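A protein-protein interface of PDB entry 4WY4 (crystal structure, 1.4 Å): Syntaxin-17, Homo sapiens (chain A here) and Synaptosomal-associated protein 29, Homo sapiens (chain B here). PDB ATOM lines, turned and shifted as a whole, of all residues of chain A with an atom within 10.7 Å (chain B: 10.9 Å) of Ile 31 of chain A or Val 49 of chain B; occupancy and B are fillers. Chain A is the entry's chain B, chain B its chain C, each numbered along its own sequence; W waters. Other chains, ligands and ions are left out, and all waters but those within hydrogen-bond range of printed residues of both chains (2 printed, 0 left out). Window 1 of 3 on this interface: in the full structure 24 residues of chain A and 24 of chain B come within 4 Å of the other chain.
O of Val 24 of chain A is in hydrogen-bond range of NE2 of Gln 46 of chain B (3.1 Å).
The side-chain amide oxygen (OE1) of Gln 28 of chain A is in hydrogen-bond range of the side-chain amide nitrogen (NE2) of Gln 46 of chain B, at 2.9 Å.
The side-chain amide nitrogen (ND2) of Asn 25 of chain A sits at hydrogen-bond distance from the side-chain carboxylate (OE2) of Glu 42 of chain B (3.0 Å).
Val 24 of chain A touches Ser 39 of chain B.
Val 24 of chain A touches Glu 42 of chain B (CG1 to OE1, 3.7 Å).
OE1 of Gln 46 of chain B touches CD1 of Ile 31 of chain A (3.3 Å).
Val 49 of chain B touches Ile 31 of chain A.
Ala 35 of chain A touches Val 49 of chain B.
Ala 35 of chain A touches Thr 53 of chain B.
Val 38 of chain A touches Thr 53 of chain B.
CB of Met 56 of chain B touches CG1 of Val 38 of chain A, 3.5 Å away.
Val 57 of chain B touches Val 38 of chain A (CG2 to CG1, 3.9 Å).
Of the 18 printed residues of chain B, 7 touch a printed residue of chain A.
Among the printed residues, 12 pairs touch across the chains.
Among the printed residues, no Asp or Glu carboxylate lies within 4 Å of a Lys or Arg side-chain nitrogen of the other chain.
The side-chain amide nitrogen (NE2) of Gln 28 of chain A sits at hydrogen-bond distance from the side-chain carboxylate (OD1) of Asp 32 of chain A (3.0 Å).
The backbone carbonyl oxygen of Val 49 of chain B sits at hydrogen-bond distance from the side-chain hydroxyl of Thr 53 of chain B, 2.7 Å away.
Water W1 lies within hydrogen-bond range of the side-chain amide nitrogen (NE2) of Gln 28 of chain A, the backbone carbonyl oxygen (O) of Arg 45 of chain B and the backbone NH (N) of Gln 46 of chain B.
Water W2 bridges the guanidinium group (NE) of Arg 45 of chain B (3.0 Å) and the side-chain amide oxygen (OE1) of Gln 28 of chain A (3.3 Å).
Printed residues of chain B within 4 Å of Ile 31 of chain A: Gln 46 (3.3 Å) and Val 49 (3.7 Å).
Printed residues of chain A within 4 Å of Val 49 of chain B: Ile 31 (3.7 Å) and Ala 35 (3.6 Å).
No residue of chain B comes within 4 Å of Asp 32 of chain A.
No residue of chain B comes within 4 Å of Ile 34 of chain A.
Ala 35 of chain A touches just these residues of chain B: Val 49 (3.6 Å) and Thr 53 (3.7 Å).
No residue of chain A comes within 4 Å of Gly 48 of chain B.
Of chain A, only Ala 35 and Val 38 come within 4 Å of Thr 53 of chain B.
Of the printed residues of chain B, Val 38 of chain A touches Thr 53, Met 56 and Val 57.
Printed residues of chain B within 4 Å of Val 24 of chain A: Ser 39 (3.8 Å), Glu 42 (3.7 Å) and Gln 46 (3.1 Å).
Of the printed residues of chain A, Glu 42 of chain B touches Val 24 (3.7 Å) and Asn 25 (3.0 Å).
Of the printed residues of chain A, Gln 46 of chain B touches Val 24, Gln 28 and Ile 31.
Of the printed residues of chain A, Ser 39 of chain B touches Val 24 (3.8 Å).
Gln 27 of chain A touches none of the printed residues of chain B.
The nearest printed residue of chain B that does not touch Ile 31 of chain A is Leu 50 of chain B (4.3 Å).
The nearest printed residue of chain A that does not touch Val 49 of chain B is Asp 32 of chain A (4.8 Å).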
ATOM      1  N   LEU A  22     -35.884  -0.060  20.643  1.00  0.00           N
ATOM      2  CA  LEU A  22     -35.589   0.094  22.077  1.00  0.00           C
ATOM      3  C   LEU A  22     -34.824  -1.108  22.614  1.00  0.00           C
ATOM      4  O   LEU A  22     -33.895  -0.970  23.432  1.00  0.00           O
ATOM      5  CB  LEU A  22     -36.883   0.303  22.885  1.00  0.00           C
ATOM      6  CG  LEU A  22     -37.524   1.666  22.604  1.00  0.00           C
ATOM      7  CD1 LEU A  22     -38.963   1.723  23.126  1.00  0.00           C
ATOM      8  CD2 LEU A  22     -36.711   2.793  23.228  1.00  0.00           C
ATOM      9  N   LEU A  23     -35.156  -2.286  22.116  1.00  0.00           N
ATOM     10  CA  LEU A  23     -34.466  -3.500  22.540  1.00  0.00           C
ATOM     11  C   LEU A  23     -33.016  -3.520  22.028  1.00  0.00           C
ATOM     12  O   LEU A  23     -32.097  -3.870  22.794  1.00  0.00           O
ATOM     13  CB  LEU A  23     -35.236  -4.733  22.060  1.00  0.00           C
ATOM     14  CG  LEU A  23     -36.541  -5.023  22.818  1.00  0.00           C
ATOM     15  CD1 LEU A  23     -37.360  -6.039  22.067  1.00  0.00           C
ATOM     16  CD2 LEU A  23     -36.248  -5.506  24.235  1.00  0.00           C
ATOM     17  N   VAL A  24     -32.796  -3.186  20.760  1.00  0.00           N
ATOM     18  CA  VAL A  24     -31.435  -3.102  20.224  1.00  0.00           C
ATOM     19  C   VAL A  24     -30.622  -2.105  21.048  1.00  0.00           C
ATOM     20  O   VAL A  24     -29.476  -2.378  21.443  1.00  0.00           O
ATOM     21  CB  VAL A  24     -31.449  -2.687  18.750  1.00  0.00           C
ATOM     22  CG1 VAL A  24     -30.063  -2.232  18.265  1.00  0.00           C
ATOM     23  CG2 VAL A  24     -32.016  -3.796  17.874  1.00  0.00           C
ATOM     24  N   ASN A  25     -31.197  -0.951  21.353  1.00  0.00           N
ATOM     25  CA  ASN A  25     -30.476   0.057  22.100  1.00  0.00           C
ATOM     26  C   ASN A  25     -30.181  -0.400  23.530  1.00  0.00           C
ATOM     27  O   ASN A  25     -29.085  -0.134  24.068  1.00  0.00           O
ATOM     28  CB  ASN A  25     -31.261   1.369  22.097  1.00  0.00           C
ATOM     29  CG  ASN A  25     -30.547   2.466  22.843  1.00  0.00           C
ATOM     30  OD1 ASN A  25     -30.908   2.793  23.967  1.00  0.00           O
ATOM     31  ND2 ASN A  25     -29.510   3.023  22.234  1.00  0.00           N
ATOM     32  N   SER A  26     -31.123  -1.125  24.129  1.00  0.00           N
ATOM     33  CA  SER A  26     -30.971  -1.586  25.500  1.00  0.00           C
ATOM     34  C   SER A  26     -29.856  -2.630  25.630  1.00  0.00           C
ATOM     35  O   SER A  26     -29.286  -2.820  26.733  1.00  0.00           O
ATOM     36  CB  SER A  26     -32.297  -2.158  26.036  1.00  0.00           C
ATOM     37  OG  SER A  26     -32.630  -3.408  25.452  1.00  0.00           O
ATOM     38  N   GLN A  27     -29.535  -3.295  24.516  1.00  0.00           N
ATOM     39  CA  GLN A  27     -28.478  -4.315  24.468  1.00  0.00           C
ATOM     40  C   GLN A  27     -27.083  -3.726  24.207  1.00  0.00           C
ATOM     41  O   GLN A  27     -26.069  -4.428  24.351  1.00  0.00           O
ATOM     42  CB  GLN A  27     -28.855  -5.361  23.413  1.00  0.00           C
ATOM     43  CG  GLN A  27     -30.080  -6.176  23.860  1.00  0.00           C
ATOM     44  CD  GLN A  27     -30.590  -7.163  22.841  1.00  0.00           C
ATOM     45  OE1 GLN A  27     -29.927  -7.463  21.840  1.00  0.00           O
ATOM     46  NE2 GLN A  27     -31.816  -7.662  23.074  1.00  0.00           N
ATOM     47  N   GLN A  28     -27.004  -2.433  23.923  1.00  0.00           N
ATOM     48  CA  GLN A  28     -25.718  -1.781  23.689  1.00  0.00           C
ATOM     49  C   GLN A  28     -24.797  -1.942  24.897  1.00  0.00           C
ATOM     50  O   GLN A  28     -23.592  -2.211  24.748  1.00  0.00           O
ATOM     51  CB  GLN A  28     -25.905  -0.294  23.387  1.00  0.00           C
ATOM     52  CG  GLN A  28     -24.567   0.382  23.026  1.00  0.00           C
ATOM     53  CD  GLN A  28     -24.013  -0.129  21.719  1.00  0.00           C
ATOM     54  OE1 GLN A  28     -24.739  -0.243  20.746  1.00  0.00           O
ATOM     55  NE2 GLN A  28     -22.724  -0.442  21.685  1.00  0.00           N
ATOM     56  N   GLU A  29     -25.319  -1.795  26.105  1.00  0.00           N
ATOM     57  CA  GLU A  29     -24.442  -1.836  27.276  1.00  0.00           C
ATOM     58  C   GLU A  29     -23.903  -3.244  27.475  1.00  0.00           C
ATOM     59  O   GLU A  29     -22.761  -3.392  27.933  1.00  0.00           O
ATOM     60  CB  GLU A  29     -25.141  -1.350  28.553  1.00  0.00           C
ATOM     61  CG  GLU A  29     -24.671   0.030  29.055  1.00  0.00           C
ATOM     62  CD  GLU A  29     -23.218   0.053  29.551  1.00  0.00           C
ATOM     63  OE1 GLU A  29     -22.930  -0.456  30.665  1.00  0.00           O
ATOM     64  OE2 GLU A  29     -22.357   0.606  28.825  1.00  0.00           O
ATOM     65  N   LYS A  30     -24.663  -4.284  27.098  1.00  0.00           N
ATOM     66  CA  LYS A  30     -24.133  -5.648  27.240  1.00  0.00           C
ATOM     67  C   LYS A  30     -22.988  -5.845  26.259  1.00  0.00           C
ATOM     68  O   LYS A  30     -21.962  -6.429  26.617  1.00  0.00           O
ATOM     69  CB  LYS A  30     -25.206  -6.732  27.018  1.00  0.00           C
ATOM     70  CG  LYS A  30     -26.147  -6.971  28.216  1.00  0.00           C
ATOM     71  CD  LYS A  30     -27.371  -7.816  27.801  1.00  0.00           C
ATOM     72  CE  LYS A  30     -28.574  -7.605  28.713  1.00  0.00           C
ATOM     73  NZ  LYS A  30     -29.669  -8.552  28.366  1.00  0.00           N
ATOM     74  N   ILE A  31     -23.132  -5.366  25.043  1.00  0.00           N
ATOM     75  CA  ILE A  31     -22.097  -5.520  24.037  1.00  0.00           C
ATOM     76  C   ILE A  31     -20.839  -4.738  24.445  1.00  0.00           C
ATOM     77  O   ILE A  31     -19.729  -5.261  24.338  1.00  0.00           O
ATOM     78  CB  ILE A  31     -22.640  -5.095  22.665  1.00  0.00           C
ATOM     79  CG1 ILE A  31     -23.742  -6.069  22.263  1.00  0.00           C
ATOM     80  CG2 ILE A  31     -21.524  -5.080  21.616  1.00  0.00           C
ATOM     81  CD1 ILE A  31     -24.581  -5.557  21.140  1.00  0.00           C
ATOM     82  N   ASP A  32     -20.991  -3.529  24.947  1.00  0.00           N
ATOM     83  CA  ASP A  32     -19.855  -2.731  25.377  1.00  0.00           C
ATOM     84  C   ASP A  32     -19.166  -3.386  26.562  1.00  0.00           C
ATOM     85  O   ASP A  32     -17.930  -3.332  26.675  1.00  0.00           O
ATOM     86  CB  ASP A  32     -20.268  -1.303  25.720  1.00  0.00           C
ATOM     87  CG  ASP A  32     -20.687  -0.516  24.478  1.00  0.00           C
ATOM     88  OD1 ASP A  32     -20.289  -0.912  23.351  1.00  0.00           O
ATOM     89  OD2 ASP A  32     -21.390   0.502  24.617  1.00  0.00           O
ATOM     90  N   SER A  33     -19.936  -3.979  27.463  1.00  0.00           N
ATOM     91  CA  SER A  33     -19.345  -4.633  28.635  1.00  0.00           C
ATOM     92  C   SER A  33     -18.559  -5.869  28.224  1.00  0.00           C
ATOM     93  O   SER A  33     -17.452  -6.095  28.737  1.00  0.00           O
ATOM     94  CB  SER A  33     -20.421  -5.022  29.661  1.00  0.00           C
ATOM     95  OG  SER A  33     -20.951  -3.860  30.245  1.00  0.00           O
ATOM     96  N   ILE A  34     -19.094  -6.682  27.337  1.00  0.00           N
ATOM     97  CA  ILE A  34     -18.377  -7.828  26.801  1.00  0.00           C
ATOM     98  C   ILE A  34     -17.072  -7.370  26.181  1.00  0.00           C
ATOM     99  O   ILE A  34     -16.004  -7.934  26.439  1.00  0.00           O
ATOM    100  CB  ILE A  34     -19.248  -8.571  25.739  1.00  0.00           C
ATOM    101  CG1 ILE A  34     -20.397  -9.292  26.432  1.00  0.00           C
ATOM    102  CG2 ILE A  34     -18.421  -9.497  24.851  1.00  0.00           C
ATOM    103  CD1 ILE A  34     -21.577  -9.588  25.474  1.00  0.00           C
ATOM    104  N   ALA A  35     -17.122  -6.340  25.378  1.00  0.00           N
ATOM    105  CA  ALA A  35     -15.928  -5.851  24.671  1.00  0.00           C
ATOM    106  C   ALA A  35     -14.894  -5.371  25.683  1.00  0.00           C
ATOM    107  O   ALA A  35     -13.689  -5.618  25.516  1.00  0.00           O
ATOM    108  CB  ALA A  35     -16.296  -4.718  23.712  1.00  0.00           C
ATOM    109  N   ASP A  36     -15.336  -4.684  26.723  1.00  0.00           N
ATOM    110  CA  ASP A  36     -14.435  -4.150  27.733  1.00  0.00           C
ATOM    111  C   ASP A  36     -13.801  -5.282  28.533  1.00  0.00           C
ATOM    112  O   ASP A  36     -12.595  -5.256  28.834  1.00  0.00           O
ATOM    113  CB  ASP A  36     -15.187  -3.190  28.656  1.00  0.00           C
ATOM    114  CG  ASP A  36     -14.364  -2.730  29.815  1.00  0.00           C
ATOM    115  OD1 ASP A  36     -13.455  -1.898  29.591  1.00  0.00           O
ATOM    116  OD2 ASP A  36     -14.672  -3.179  30.939  1.00  0.00           O
ATOM    117  N   HIS A  37     -14.592  -6.268  28.941  1.00  0.00           N
ATOM    118  CA  HIS A  37     -14.034  -7.407  29.678  1.00  0.00           C
ATOM    119  C   HIS A  37     -12.988  -8.108  28.829  1.00  0.00           C
ATOM    120  O   HIS A  37     -11.908  -8.483  29.332  1.00  0.00           O
ATOM    121  CB  HIS A  37     -15.107  -8.454  30.023  1.00  0.00           C
ATOM    122  CG  HIS A  37     -15.994  -8.107  31.174  1.00  0.00           C
ATOM    123  ND1 HIS A  37     -15.533  -7.734  32.414  1.00  0.00           N
ATOM    124  CD2 HIS A  37     -17.353  -8.122  31.273  1.00  0.00           C
ATOM    125  CE1 HIS A  37     -16.559  -7.568  33.249  1.00  0.00           C
ATOM    126  NE2 HIS A  37     -17.681  -7.773  32.564  1.00  0.00           N
ATOM    127  N   VAL A  38     -13.270  -8.343  27.565  1.00  0.00           N
ATOM    128  CA  VAL A  38     -12.342  -9.035  26.676  1.00  0.00           C
ATOM    129  C   VAL A  38     -11.094  -8.186  26.443  1.00  0.00           C
ATOM    130  O   VAL A  38      -9.960  -8.726  26.438  1.00  0.00           O
ATOM    131  CB  VAL A  38     -13.027  -9.395  25.337  1.00  0.00           C
ATOM    132  CG1 VAL A  38     -11.985  -9.782  24.268  1.00  0.00           C
ATOM    133  CG2 VAL A  38     -14.004 -10.549  25.610  1.00  0.00           C
ATOM    134  N   ASN A  39     -11.238  -6.884  26.280  1.00  0.00           N
ATOM    135  CA  ASN A  39     -10.081  -6.013  26.122  1.00  0.00           C
ATOM    136  C   ASN A  39      -9.159  -6.090  27.344  1.00  0.00           C
ATOM    137  O   ASN A  39      -7.929  -6.201  27.213  1.00  0.00           O
ATOM    138  CB  ASN A  39     -10.519  -4.577  25.930  1.00  0.00           C
ATOM    139  CG  ASN A  39      -9.356  -3.675  25.711  1.00  0.00           C
ATOM    140  OD1 ASN A  39      -8.808  -3.651  24.624  1.00  0.00           O
ATOM    141  ND2 ASN A  39      -8.955  -2.940  26.740  1.00  0.00           N
ATOM    142  N   SER B  39     -32.175   1.932  13.606  1.00  0.00           N
ATOM    143  CA  SER B  39     -31.943   0.724  14.380  1.00  0.00           C
ATOM    144  C   SER B  39     -31.065  -0.258  13.620  1.00  0.00           C
ATOM    145  O   SER B  39     -30.205  -0.927  14.201  1.00  0.00           O
ATOM    146  CB  SER B  39     -33.289   0.080  14.724  1.00  0.00           C
ATOM    147  OG  SER B  39     -33.065  -1.040  15.549  1.00  0.00           O
ATOM    148  N   GLU B  41     -28.748   0.554  11.496  1.00  0.00           N
ATOM    149  CA  GLU B  41     -27.403   1.129  11.550  1.00  0.00           C
ATOM    150  C   GLU B  41     -26.785   0.845  12.907  1.00  0.00           C
ATOM    151  O   GLU B  41     -25.596   0.508  13.014  1.00  0.00           O
ATOM    152  CB  GLU B  41     -27.443   2.629  11.275  1.00  0.00           C
ATOM    153  CG  GLU B  41     -27.848   2.965   9.835  1.00  0.00           C
ATOM    154  CD  GLU B  41     -28.116   4.442   9.610  1.00  0.00           C
ATOM    155  OE1 GLU B  41     -28.324   5.181  10.599  1.00  0.00           O
ATOM    156  OE2 GLU B  41     -28.117   4.864   8.436  1.00  0.00           O
ATOM    157  N   GLU B  42     -27.581   0.903  13.965  1.00  0.00           N
ATOM    158  CA  GLU B  42     -27.090   0.601  15.306  1.00  0.00           C
ATOM    159  C   GLU B  42     -26.712  -0.873  15.419  1.00  0.00           C
ATOM    160  O   GLU B  42     -25.683  -1.220  16.010  1.00  0.00           O
ATOM    161  CB  GLU B  42     -28.144   0.956  16.356  1.00  0.00           C
ATOM    162  CG  GLU B  42     -27.663   0.768  17.782  1.00  0.00           C
ATOM    163  CD  GLU B  42     -28.626   1.341  18.793  1.00  0.00           C
ATOM    164  OE1 GLU B  42     -29.825   1.447  18.463  1.00  0.00           O
ATOM    165  OE2 GLU B  42     -28.179   1.695  19.904  1.00  0.00           O
ATOM    166  N   LEU B  43     -27.540  -1.757  14.872  1.00  0.00           N
ATOM    167  CA  LEU B  43     -27.242  -3.189  14.822  1.00  0.00           C
ATOM    168  C   LEU B  43     -25.917  -3.434  14.127  1.00  0.00           C
ATOM    169  O   LEU B  43     -25.098  -4.256  14.587  1.00  0.00           O
ATOM    170  CB  LEU B  43     -28.334  -3.935  14.054  1.00  0.00           C
ATOM    171  CG  LEU B  43     -29.357  -4.722  14.838  1.00  0.00           C
ATOM    172  CD1 LEU B  43     -30.192  -5.529  13.846  1.00  0.00           C
ATOM    173  CD2 LEU B  43     -28.771  -5.625  15.903  1.00  0.00           C
ATOM    174  N   ALA B  44     -25.705  -2.761  13.007  1.00  0.00           N
ATOM    175  CA  ALA B  44     -24.468  -2.952  12.251  1.00  0.00           C
ATOM    176  C   ALA B  44     -23.249  -2.491  13.044  1.00  0.00           C
ATOM    177  O   ALA B  44     -22.190  -3.139  13.017  1.00  0.00           O
ATOM    178  CB  ALA B  44     -24.545  -2.226  10.921  1.00  0.00           C
ATOM    179  N   ARG B  45     -23.379  -1.387  13.768  1.00  0.00           N
ATOM    180  CA  ARG B  45     -22.291  -0.937  14.640  1.00  0.00           C
ATOM    181  C   ARG B  45     -21.992  -1.976  15.705  1.00  0.00           C
ATOM    182  O   ARG B  45     -20.809  -2.241  16.045  1.00  0.00           O
ATOM    183  CB  ARG B  45     -22.638   0.393  15.286  1.00  0.00           C
ATOM    184  CG  ARG B  45     -22.549   1.579  14.327  1.00  0.00           C
ATOM    185  CD  ARG B  45     -22.590   2.927  15.049  1.00  0.00           C
ATOM    186  NE  ARG B  45     -23.854   3.177  15.742  1.00  0.00           N
ATOM    187  CZ  ARG B  45     -24.919   3.733  15.174  1.00  0.00           C
ATOM    188  NH1 ARG B  45     -26.014   3.937  15.886  1.00  0.00           N
ATOM    189  NH2 ARG B  45     -24.872   4.079  13.899  1.00  0.00           N
ATOM    190  N   GLN B  46     -23.041  -2.567  16.272  1.00  0.00           N
ATOM    191  CA  GLN B  46     -22.843  -3.574  17.302  1.00  0.00           C
ATOM    192  C   GLN B  46     -22.121  -4.792  16.735  1.00  0.00           C
ATOM    193  O   GLN B  46     -21.270  -5.391  17.419  1.00  0.00           O
ATOM    194  CB  GLN B  46     -24.200  -3.973  17.900  1.00  0.00           C
ATOM    195  CG  GLN B  46     -24.772  -2.833  18.760  1.00  0.00           C
ATOM    196  CD  GLN B  46     -26.166  -3.145  19.290  1.00  0.00           C
ATOM    197  OE1 GLN B  46     -26.728  -4.204  18.998  1.00  0.00           O
ATOM    198  NE2 GLN B  46     -26.696  -2.249  20.113  1.00  0.00           N
ATOM    199  N   ARG B  47     -22.410  -5.172  15.497  1.00  0.00           N
ATOM    200  CA  ARG B  47     -21.684  -6.277  14.872  1.00  0.00           C
ATOM    201  C   ARG B  47     -20.180  -5.967  14.773  1.00  0.00           C
ATOM    202  O   ARG B  47     -19.352  -6.835  15.018  1.00  0.00           O
ATOM    203  CB  ARG B  47     -22.253  -6.605  13.482  1.00  0.00           C
ATOM    204  CG  ARG B  47     -21.395  -7.629  12.730  1.00  0.00           C
ATOM    205  CD  ARG B  47     -22.136  -8.329  11.625  1.00  0.00           C
ATOM    206  NE  ARG B  47     -22.856  -7.375  10.802  1.00  0.00           N
ATOM    207  CZ  ARG B  47     -22.291  -6.529   9.947  1.00  0.00           C
ATOM    208  NH1 ARG B  47     -20.967  -6.531   9.775  1.00  0.00           N
ATOM    209  NH2 ARG B  47     -23.060  -5.689   9.250  1.00  0.00           N
ATOM    210  N   GLY B  48     -19.832  -4.728  14.451  1.00  0.00           N
ATOM    211  CA  GLY B  48     -18.431  -4.337  14.364  1.00  0.00           C
ATOM    212  C   GLY B  48     -17.753  -4.521  15.713  1.00  0.00           C
ATOM    213  O   GLY B  48     -16.610  -4.977  15.783  1.00  0.00           O
ATOM    214  N   VAL B  49     -18.433  -4.208  16.809  1.00  0.00           N
ATOM    215  CA  VAL B  49     -17.830  -4.421  18.117  1.00  0.00           C
ATOM    216  C   VAL B  49     -17.652  -5.903  18.402  1.00  0.00           C
ATOM    217  O   VAL B  49     -16.608  -6.327  18.952  1.00  0.00           O
ATOM    218  CB  VAL B  49     -18.688  -3.783  19.233  1.00  0.00           C
ATOM    219  CG1 VAL B  49     -18.123  -4.145  20.614  1.00  0.00           C
ATOM    220  CG2 VAL B  49     -18.729  -2.270  19.039  1.00  0.00           C
ATOM    221  N   LEU B  50     -18.633  -6.729  18.053  1.00  0.00           N
ATOM    222  CA  LEU B  50     -18.505  -8.166  18.253  1.00  0.00           C
ATOM    223  C   LEU B  50     -17.386  -8.745  17.420  1.00  0.00           C
ATOM    224  O   LEU B  50     -16.642  -9.621  17.900  1.00  0.00           O
ATOM    225  CB  LEU B  50     -19.821  -8.875  17.904  1.00  0.00           C
ATOM    226  CG  LEU B  50     -20.966  -8.607  18.883  1.00  0.00           C
ATOM    227  CD1 LEU B  50     -22.259  -9.269  18.369  1.00  0.00           C
ATOM    228  CD2 LEU B  50     -20.610  -9.115  20.274  1.00  0.00           C
ATOM    229  N   GLU B  51     -17.213  -8.252  16.194  1.00  0.00           N
ATOM    230  CA  GLU B  51     -16.156  -8.755  15.314  1.00  0.00           C
ATOM    231  C   GLU B  51     -14.764  -8.411  15.885  1.00  0.00           C
ATOM    232  O   GLU B  51     -13.830  -9.239  15.864  1.00  0.00           O
ATOM    233  CB  GLU B  51     -16.334  -8.183  13.897  1.00  0.00           C
ATOM    234  CG  GLU B  51     -17.515  -8.811  13.123  1.00  0.00           C
ATOM    235  CD  GLU B  51     -17.859  -8.061  11.847  1.00  0.00           C
ATOM    236  OE1 GLU B  51     -17.312  -6.958  11.624  1.00  0.00           O
ATOM    237  OE2 GLU B  51     -18.681  -8.581  11.055  1.00  0.00           O
ATOM    238  N   ARG B  52     -14.617  -7.200  16.394  1.00  0.00           N
ATOM    239  CA  ARG B  52     -13.362  -6.803  17.019  1.00  0.00           C
ATOM    240  C   ARG B  52     -13.111  -7.662  18.252  1.00  0.00           C
ATOM    241  O   ARG B  52     -11.971  -8.095  18.517  1.00  0.00           O
ATOM    242  CB  ARG B  52     -13.374  -5.328  17.398  1.00  0.00           C
ATOM    243  CG  ARG B  52     -12.102  -4.904  18.122  1.00  0.00           C
ATOM    244  CD  ARG B  52     -12.063  -3.396  18.352  1.00  0.00           C
ATOM    245  NE  ARG B  52     -12.237  -2.649  17.109  1.00  0.00           N
ATOM    246  CZ  ARG B  52     -13.335  -1.975  16.768  1.00  0.00           C
ATOM    247  NH1 ARG B  52     -14.382  -1.920  17.587  1.00  0.00           N
ATOM    248  NH2 ARG B  52     -13.374  -1.337  15.603  1.00  0.00           N
ATOM    249  N   THR B  53     -14.168  -7.925  19.022  1.00  0.00           N
ATOM    250  CA  THR B  53     -14.043  -8.735  20.219  1.00  0.00           C
ATOM    251  C   THR B  53     -13.550 -10.125  19.873  1.00  0.00           C
ATOM    252  O   THR B  53     -12.692 -10.688  20.578  1.00  0.00           O
ATOM    253  CB  THR B  53     -15.407  -8.801  20.963  1.00  0.00           C
ATOM    254  OG1 THR B  53     -15.804  -7.477  21.308  1.00  0.00           O
ATOM    255  CG2 THR B  53     -15.285  -9.607  22.253  1.00  0.00           C
ATOM    256  N   GLU B  54     -14.054 -10.705  18.785  1.00  0.00           N
ATOM    257  CA  GLU B  54     -13.595 -12.027  18.367  1.00  0.00           C
ATOM    258  C   GLU B  54     -12.111 -11.995  17.995  1.00  0.00           C
ATOM    259  O   GLU B  54     -11.379 -12.928  18.349  1.00  0.00           O
ATOM    260  CB  GLU B  54     -14.439 -12.579  17.211  1.00  0.00           C
ATOM    261  CG  GLU B  54     -14.068 -14.018  16.876  1.00  0.00           C
ATOM    262  CD  GLU B  54     -14.960 -14.643  15.853  1.00  0.00           C
ATOM    263  OE1 GLU B  54     -15.814 -13.946  15.241  1.00  0.00           O
ATOM    264  OE2 GLU B  54     -14.802 -15.846  15.649  1.00  0.00           O
ATOM    265  N   LYS B  55     -11.639 -10.930  17.356  1.00  0.00           N
ATOM    266  CA  LYS B  55     -10.196 -10.818  17.071  1.00  0.00           C
ATOM    267  C   LYS B  55      -9.383 -10.768  18.352  1.00  0.00           C
ATOM    268  O   LYS B  55      -8.269 -11.309  18.395  1.00  0.00           O
ATOM    269  CB  LYS B  55      -9.904  -9.578  16.244  1.00  0.00           C
ATOM    270  CG  LYS B  55     -10.513  -9.620  14.861  1.00  0.00           C
ATOM    271  CD  LYS B  55     -10.218  -8.317  14.154  1.00  0.00           C
ATOM    272  CE  LYS B  55     -10.920  -8.224  12.835  1.00  0.00           C
ATOM    273  NZ  LYS B  55     -10.777  -6.872  12.233  1.00  0.00           N
ATOM    274  N   MET B  56      -9.909 -10.161  19.411  1.00  0.00           N
ATOM    275  CA  MET B  56      -9.167 -10.091  20.660  1.00  0.00           C
ATOM    276  C   MET B  56      -9.132 -11.450  21.335  1.00  0.00           C
ATOM    277  O   MET B  56      -8.133 -11.789  21.994  1.00  0.00           O
ATOM    278  CB  MET B  56      -9.784  -9.050  21.602  1.00  0.00           C
ATOM    279  CG  MET B  56      -9.799  -7.631  21.069  1.00  0.00           C
ATOM    280  SD  MET B  56      -8.157  -6.999  20.685  1.00  0.00           S
ATOM    281  CE  MET B  56      -7.530  -6.809  22.296  1.00  0.00           C
ATOM    282  N   VAL B  57     -10.196 -12.248  21.260  1.00  0.00           N
ATOM    283  CA  VAL B  57     -10.183 -13.587  21.829  1.00  0.00           C
ATOM    284  C   VAL B  57      -9.201 -14.470  21.063  1.00  0.00           C
ATOM    285  O   VAL B  57      -8.467 -15.261  21.656  1.00  0.00           O
ATOM    286  CB  VAL B  57     -11.608 -14.188  21.826  1.00  0.00           C
ATOM    287  CG1 VAL B  57     -11.594 -15.623  22.347  1.00  0.00           C
ATOM    288  CG2 VAL B  57     -12.527 -13.313  22.678  1.00  0.00           C
HETATM  289  O   HOH W   1     -21.841  -0.526  18.802  1.00  0.00           O
HETATM  290  O   HOH W   2     -23.505   1.655  18.355  1.00  0.00           O
